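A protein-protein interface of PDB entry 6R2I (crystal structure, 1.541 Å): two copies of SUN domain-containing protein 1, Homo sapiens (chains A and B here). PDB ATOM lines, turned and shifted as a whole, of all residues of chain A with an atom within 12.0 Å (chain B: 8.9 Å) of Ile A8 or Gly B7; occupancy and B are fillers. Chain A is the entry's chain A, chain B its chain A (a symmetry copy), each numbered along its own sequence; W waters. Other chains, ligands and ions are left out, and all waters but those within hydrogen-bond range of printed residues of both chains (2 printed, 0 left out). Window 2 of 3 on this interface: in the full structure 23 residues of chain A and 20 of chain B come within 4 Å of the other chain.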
ATOM      1  N   GLY A   6     -10.770   0.140  11.393  1.00  0.00           N
ATOM      2  CA  GLY A   6     -10.755   0.486  12.805  1.00  0.00           C
ATOM      3  C   GLY A   6      -9.593  -0.044  13.638  1.00  0.00           C
ATOM      4  O   GLY A   6      -9.087   0.675  14.507  1.00  0.00           O
ATOM      5  N   GLY A   7      -9.166  -1.309  13.395  1.00  0.00           N
ATOM      6  CA  GLY A   7      -8.094  -1.908  14.183  1.00  0.00           C
ATOM      7  C   GLY A   7      -6.716  -1.772  13.544  1.00  0.00           C
ATOM      8  O   GLY A   7      -6.581  -1.551  12.347  1.00  0.00           O
ATOM      9  N   ILE A   8      -5.673  -1.959  14.359  1.00  0.00           N
ATOM     10  CA  ILE A   8      -4.290  -1.767  13.923  1.00  0.00           C
ATOM     11  C   ILE A   8      -3.628  -3.117  13.682  1.00  0.00           C
ATOM     12  O   ILE A   8      -4.014  -4.139  14.262  1.00  0.00           O
ATOM     13  CB  ILE A   8      -3.473  -0.914  14.921  1.00  0.00           C
ATOM     14  CG1 ILE A   8      -3.326  -1.564  16.304  1.00  0.00           C
ATOM     15  CG2 ILE A   8      -4.074   0.464  15.029  1.00  0.00           C
ATOM     16  CD1 ILE A   8      -2.078  -1.018  17.073  1.00  0.00           C
ATOM     17  N   THR A   9      -2.631  -3.124  12.803  1.00  0.00           N
ATOM     18  CA  THR A   9      -1.862  -4.315  12.493  1.00  0.00           C
ATOM     19  C   THR A   9      -0.674  -4.452  13.446  1.00  0.00           C
ATOM     20  O   THR A   9      -0.293  -3.514  14.151  1.00  0.00           O
ATOM     21  CB  THR A   9      -1.303  -4.269  11.063  1.00  0.00           C
ATOM     22  OG1 THR A   9      -0.315  -3.221  10.965  1.00  0.00           O
ATOM     23  CG2 THR A   9      -2.417  -4.070  10.030  1.00  0.00           C
ATOM     24  N   GLU A  10      -0.048  -5.636  13.414  1.00  0.00           N
ATOM     25  CA  GLU A  10       1.167  -5.865  14.204  1.00  0.00           C
ATOM     26  C   GLU A  10       2.279  -4.891  13.817  1.00  0.00           C
ATOM     27  O   GLU A  10       2.946  -4.314  14.701  1.00  0.00           O
ATOM     28  CB  GLU A  10       1.632  -7.330  14.044  1.00  0.00           C
ATOM     29  CG  GLU A  10       2.931  -7.633  14.841  1.00  0.00           C
ATOM     30  CD  GLU A  10       3.501  -9.047  14.688  1.00  0.00           C
ATOM     31  OE1 GLU A  10       2.736 -10.010  14.407  1.00  0.00           O
ATOM     32  OE2 GLU A  10       4.746  -9.175  14.867  1.00  0.00           O
ATOM     33  N   ALA A  11       2.478  -4.655  12.507  1.00  0.00           N
ATOM     34  CA  ALA A  11       3.511  -3.711  12.076  1.00  0.00           C
ATOM     35  C   ALA A  11       3.241  -2.310  12.619  1.00  0.00           C
ATOM     36  O   ALA A  11       4.168  -1.619  13.085  1.00  0.00           O
ATOM     37  CB  ALA A  11       3.590  -3.706  10.544  1.00  0.00           C
ATOM     38  N   GLN A  12       1.974  -1.887  12.605  1.00  0.00           N
ATOM     39  CA  GLN A  12       1.621  -0.559  13.123  1.00  0.00           C
ATOM     40  C   GLN A  12       1.863  -0.450  14.621  1.00  0.00           C
ATOM     41  O   GLN A  12       2.319   0.604  15.109  1.00  0.00           O
ATOM     42  CB  GLN A  12       0.168  -0.238  12.774  1.00  0.00           C
ATOM     43  CG  GLN A  12      -0.016   0.021  11.278  1.00  0.00           C
ATOM     44  CD  GLN A  12      -1.463   0.140  10.820  1.00  0.00           C
ATOM     45  OE1 GLN A  12      -2.394  -0.452  11.378  1.00  0.00           O
ATOM     46  NE2 GLN A  12      -1.644   0.913   9.778  1.00  0.00           N
ATOM     47  N   ALA A  13       1.534  -1.501  15.380  1.00  0.00           N
ATOM     48  CA  ALA A  13       1.787  -1.487  16.815  1.00  0.00           C
ATOM     49  C   ALA A  13       3.282  -1.424  17.118  1.00  0.00           C
ATOM     50  O   ALA A  13       3.718  -0.690  18.020  1.00  0.00           O
ATOM     51  CB  ALA A  13       1.152  -2.729  17.454  1.00  0.00           C
ATOM     52  N   ARG A  14       4.091  -2.199  16.380  1.00  0.00           N
ATOM     53  CA  ARG A  14       5.539  -2.149  16.574  1.00  0.00           C
ATOM     54  C   ARG A  14       6.080  -0.748  16.303  1.00  0.00           C
ATOM     55  O   ARG A  14       6.952  -0.250  17.038  1.00  0.00           O
ATOM     56  CB  ARG A  14       6.220  -3.189  15.668  1.00  0.00           C
ATOM     57  CG  ARG A  14       6.052  -4.628  16.158  1.00  0.00           C
ATOM     58  CD  ARG A  14       6.669  -5.654  15.172  1.00  0.00           C
ATOM     59  NE  ARG A  14       6.515  -7.032  15.609  1.00  0.00           N
ATOM     60  CZ  ARG A  14       7.352  -7.648  16.430  1.00  0.00           C
ATOM     61  NH1 ARG A  14       8.433  -7.003  16.871  1.00  0.00           N
ATOM     62  NH2 ARG A  14       7.117  -8.906  16.787  1.00  0.00           N
ATOM     63  N   ALA A  15       5.573  -0.089  15.259  1.00  0.00           N
ATOM     64  CA  ALA A  15       6.056   1.265  14.968  1.00  0.00           C
ATOM     65  C   ALA A  15       5.688   2.261  16.074  1.00  0.00           C
ATOM     66  O   ALA A  15       6.499   3.134  16.405  1.00  0.00           O
ATOM     67  CB  ALA A  15       5.510   1.722  13.619  1.00  0.00           C
ATOM     68  N   ILE A  16       4.471   2.159  16.630  1.00  0.00           N
ATOM     69  CA  ILE A  16       4.052   3.020  17.751  1.00  0.00           C
ATOM     70  C   ILE A  16       4.952   2.807  18.979  1.00  0.00           C
ATOM     71  O   ILE A  16       5.415   3.766  19.626  1.00  0.00           O
ATOM     72  CB  ILE A  16       2.562   2.754  18.074  1.00  0.00           C
ATOM     73  CG1 ILE A  16       1.652   3.275  16.956  1.00  0.00           C
ATOM     74  CG2 ILE A  16       2.114   3.338  19.430  1.00  0.00           C
ATOM     75  CD1 ILE A  16       0.215   2.731  17.026  1.00  0.00           C
ATOM     76  N   VAL A  17       5.222   1.547  19.316  1.00  0.00           N
ATOM     77  CA  VAL A  17       6.097   1.233  20.455  1.00  0.00           C
ATOM     78  C   VAL A  17       7.493   1.800  20.238  1.00  0.00           C
ATOM     79  O   VAL A  17       8.102   2.421  21.143  1.00  0.00           O
ATOM     80  CB  VAL A  17       6.133  -0.299  20.650  1.00  0.00           C
ATOM     81  CG1 VAL A  17       7.127  -0.692  21.654  1.00  0.00           C
ATOM     82  CG2 VAL A  17       4.762  -0.789  21.036  1.00  0.00           C
ATOM     83  N   ASN A  18       8.057   1.558  19.049  1.00  0.00           N
ATOM     84  CA  ASN A  18       9.428   1.985  18.796  1.00  0.00           C
ATOM     85  C   ASN A  18       9.552   3.510  18.829  1.00  0.00           C
ATOM     86  O   ASN A  18      10.553   4.053  19.358  1.00  0.00           O
ATOM     87  CB  ASN A  18       9.905   1.382  17.475  1.00  0.00           C
ATOM     88  CG  ASN A  18      10.113  -0.161  17.544  1.00  0.00           C
ATOM     89  OD1 ASN A  18      10.183  -0.776  18.618  1.00  0.00           O
ATOM     90  ND2 ASN A  18      10.160  -0.786  16.384  1.00  0.00           N
ATOM     91  N   SER A  19       8.547   4.225  18.299  1.00  0.00           N
ATOM     92  CA  SER A  19       8.578   5.689  18.326  1.00  0.00           C
ATOM     93  C   SER A  19       8.497   6.218  19.754  1.00  0.00           C
ATOM     94  O   SER A  19       9.194   7.184  20.115  1.00  0.00           O
ATOM     95  CB  SER A  19       7.423   6.249  17.494  1.00  0.00           C
ATOM     96  OG  SER A  19       7.629   6.046  16.103  1.00  0.00           O
ATOM     97  N   ALA A  20       7.658   5.595  20.586  1.00  0.00           N
ATOM     98  CA  ALA A  20       7.553   6.020  21.986  1.00  0.00           C
ATOM     99  C   ALA A  20       8.845   5.796  22.758  1.00  0.00           C
ATOM    100  O   ALA A  20       9.246   6.656  23.567  1.00  0.00           O
ATOM    101  CB  ALA A  20       6.402   5.284  22.670  1.00  0.00           C
ATOM    102  N   GLY B   6      -6.091  -9.844  10.285  1.00  0.00           N
ATOM    103  CA  GLY B   6      -5.281  -8.658  10.055  1.00  0.00           C
ATOM    104  C   GLY B   6      -4.922  -7.815  11.274  1.00  0.00           C
ATOM    105  O   GLY B   6      -3.794  -7.317  11.361  1.00  0.00           O
ATOM    106  N   GLY B   7      -5.878  -7.631  12.220  1.00  0.00           N
ATOM    107  CA  GLY B   7      -5.631  -6.797  13.390  1.00  0.00           C
ATOM    108  C   GLY B   7      -5.168  -7.580  14.614  1.00  0.00           C
ATOM    109  O   GLY B   7      -5.366  -8.784  14.719  1.00  0.00           O
ATOM    110  N   ILE B   8      -4.582  -6.864  15.579  1.00  0.00           N
ATOM    111  CA  ILE B   8      -3.997  -7.479  16.770  1.00  0.00           C
ATOM    112  C   ILE B   8      -4.922  -7.287  17.963  1.00  0.00           C
ATOM    113  O   ILE B   8      -5.720  -6.344  18.018  1.00  0.00           O
ATOM    114  CB  ILE B   8      -2.578  -6.941  17.071  1.00  0.00           C
ATOM    115  CG1 ILE B   8      -2.548  -5.440  17.390  1.00  0.00           C
ATOM    116  CG2 ILE B   8      -1.652  -7.272  15.929  1.00  0.00           C
ATOM    117  CD1 ILE B   8      -1.285  -5.049  18.227  1.00  0.00           C
ATOM    118  N   THR B   9      -4.827  -8.203  18.922  1.00  0.00           N
ATOM    119  CA  THR B   9      -5.601  -8.145  20.148  1.00  0.00           C
ATOM    120  C   THR B   9      -4.862  -7.333  21.212  1.00  0.00           C
ATOM    121  O   THR B   9      -3.666  -7.053  21.104  1.00  0.00           O
ATOM    122  CB  THR B   9      -5.849  -9.546  20.726  1.00  0.00           C
ATOM    123  OG1 THR B   9      -4.598 -10.113  21.170  1.00  0.00           O
ATOM    124  CG2 THR B   9      -6.535 -10.461  19.707  1.00  0.00           C
ATOM    125  N   GLU B  10      -5.589  -7.003  22.289  1.00  0.00           N
ATOM    126  CA  GLU B  10      -4.975  -6.312  23.428  1.00  0.00           C
ATOM    127  C   GLU B  10      -3.838  -7.134  24.034  1.00  0.00           C
ATOM    128  O   GLU B  10      -2.753  -6.589  24.327  1.00  0.00           O
ATOM    129  CB  GLU B  10      -6.049  -5.986  24.489  1.00  0.00           C
ATOM    130  CG  GLU B  10      -5.458  -5.271  25.735  1.00  0.00           C
ATOM    131  CD  GLU B  10      -6.443  -4.966  26.868  1.00  0.00           C
ATOM    132  OE1 GLU B  10      -7.669  -4.803  26.613  1.00  0.00           O
ATOM    133  OE2 GLU B  10      -5.956  -4.881  28.032  1.00  0.00           O
ATOM    134  N   GLN B  12      -1.922  -9.303  22.545  1.00  0.00           N
ATOM    135  CA  GLN B  12      -0.782  -9.260  21.620  1.00  0.00           C
ATOM    136  C   GLN B  12      -0.041  -7.933  21.691  1.00  0.00           C
ATOM    137  O   GLN B  12       1.204  -7.904  21.615  1.00  0.00           O
ATOM    138  CB  GLN B  12      -1.260  -9.549  20.198  1.00  0.00           C
ATOM    139  CG  GLN B  12      -1.671 -11.011  20.020  1.00  0.00           C
ATOM    140  CD  GLN B  12      -2.354 -11.331  18.698  1.00  0.00           C
ATOM    141  OE1 GLN B  12      -3.034 -10.506  18.078  1.00  0.00           O
ATOM    142  NE2 GLN B  12      -2.171 -12.556  18.271  1.00  0.00           N
ATOM    143  N   ALA B  13      -0.774  -6.820  21.798  1.00  0.00           N
ATOM    144  CA  ALA B  13      -0.129  -5.518  21.925  1.00  0.00           C
ATOM    145  C   ALA B  13       0.668  -5.413  23.222  1.00  0.00           C
ATOM    146  O   ALA B  13       1.791  -4.882  23.238  1.00  0.00           O
ATOM    147  CB  ALA B  13      -1.194  -4.416  21.846  1.00  0.00           C
ATOM    148  N   ILE B  16       3.962  -7.270  22.780  1.00  0.00           N
ATOM    149  CA  ILE B  16       4.908  -6.493  21.957  1.00  0.00           C
ATOM    150  C   ILE B  16       5.562  -5.370  22.777  1.00  0.00           C
ATOM    151  O   ILE B  16       6.790  -5.159  22.737  1.00  0.00           O
ATOM    152  CB  ILE B  16       4.173  -5.945  20.709  1.00  0.00           C
ATOM    153  CG1 ILE B  16       3.810  -7.075  19.740  1.00  0.00           C
ATOM    154  CG2 ILE B  16       4.963  -4.849  19.963  1.00  0.00           C
ATOM    155  CD1 ILE B  16       2.776  -6.669  18.677  1.00  0.00           C
ATOM    156  N   VAL B  17       4.756  -4.634  23.541  1.00  0.00           N
ATOM    157  CA  VAL B  17       5.284  -3.554  24.388  1.00  0.00           C
ATOM    158  C   VAL B  17       6.266  -4.102  25.414  1.00  0.00           C
ATOM    159  O   VAL B  17       7.369  -3.546  25.633  1.00  0.00           O
ATOM    160  CB  VAL B  17       4.101  -2.829  25.068  1.00  0.00           C
ATOM    161  CG1 VAL B  17       4.564  -1.859  26.064  1.00  0.00           C
ATOM    162  CG2 VAL B  17       3.255  -2.155  24.020  1.00  0.00           C
HETATM  163  O   HOH W   1      -1.395  -7.976  12.288  1.00  0.00           O
HETATM  164  O   HOH W   2      -6.516  -4.508  15.822  1.00  0.00           O
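Ile A8 touches its own counterpart, Ile B8.
Glu A10 touches Ile B8, but with the chains exchanged Ile A8 does not touch Glu B10 (8.4 Å).
Glu A10 touches Ile B16, but with the chains exchanged Ile A16 does not touch Glu B10 (12.1 Å).
Val A17 touches its own counterpart, Val B17.
Positions printed for both chains: 6, 7, 8, 9, 10, 12, 13, 16 and 17.
Of the 9 pairs that touch across the chains among the printed residues, 2 have their exchanged pair printed and touching as well.
Of the 9 printed residues of chain B, 5 touch a printed residue of chain A.
Hydrophobic or aromatic side chains of chain A that line the printed part of chain B: Ala A13 and Val A17.
Gly B7 touches Ile A8 (CA to O, 3.2 Å).
O of Gly B6 touches CA of Thr A9, 3.7 Å away.
Thr A9 touches Ile B8 (C to CG2, 3.9 Å).
Ile B8 touches Glu A10 (CG2 to N, 3.4 Å).
CG of Glu A10 touches CD1 of Ile B16, at 3.96 Å.
CB of Ala A13 touches CD1 of Ile B8 (3.5 Å).
CG2 of Ile B16 touches CG of Arg A14, 3.96 Å away.
Val A17 touches Val B17 (CG2 to CG2, 3.6 Å).
Water W1 bridges O of Gly B6 and N of Glu A10.
Water W2 lies within hydrogen-bond range of the backbone carbonyl oxygen of Ile B8 (3.0 Å) and the backbone carbonyl oxygen of Ile A8 (3.0 Å).
Of chain B, only Gly B7 and Ile B8 come within 4 Å of Ile A8.
Of the printed residues of chain B, Ala A13 touches Ile B8.
Of the printed residues of chain B, Val A17 touches Val B17.
Gly B6 touches just one residue of chain A: Thr A9 (3.7 Å).
Gly B7 touches just one residue of chain A: Ile A8.
Ile B8 touches just these residues of chain A: Ile A8, Thr A9, Glu A10 and Ala A13.
Of the printed residues of chain A, Ile B16 touches Glu A10 and Arg A14.
Of the printed residues of chain A, Val B17 touches Val A17.
The nearest residue of chain A that does not touch Gly B7 is Thr A9 (4.6 Å).
The nearest printed residue of chain B that does not touch Arg A14 is Ile B8 (6.4 Å).
N of Ala A11 sits close to OG1 of Thr A9 (3.5 Å).
The guanidinium group (NE) of Arg A14 lies within salt-bridge range of the side-chain carboxylate (OE2) of Glu A10 (2.9 Å).
N of Thr A9 is in hydrogen-bond range of OE1 of Gln A12, 3.0 Å away.
O of Arg A14 sits close to ND2 of Asn A18, 3.3 Å away.
The backbone carbonyl oxygen of Ile A8 is in hydrogen-bond range of the backbone NH of Ile B8 (3.1 Å).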
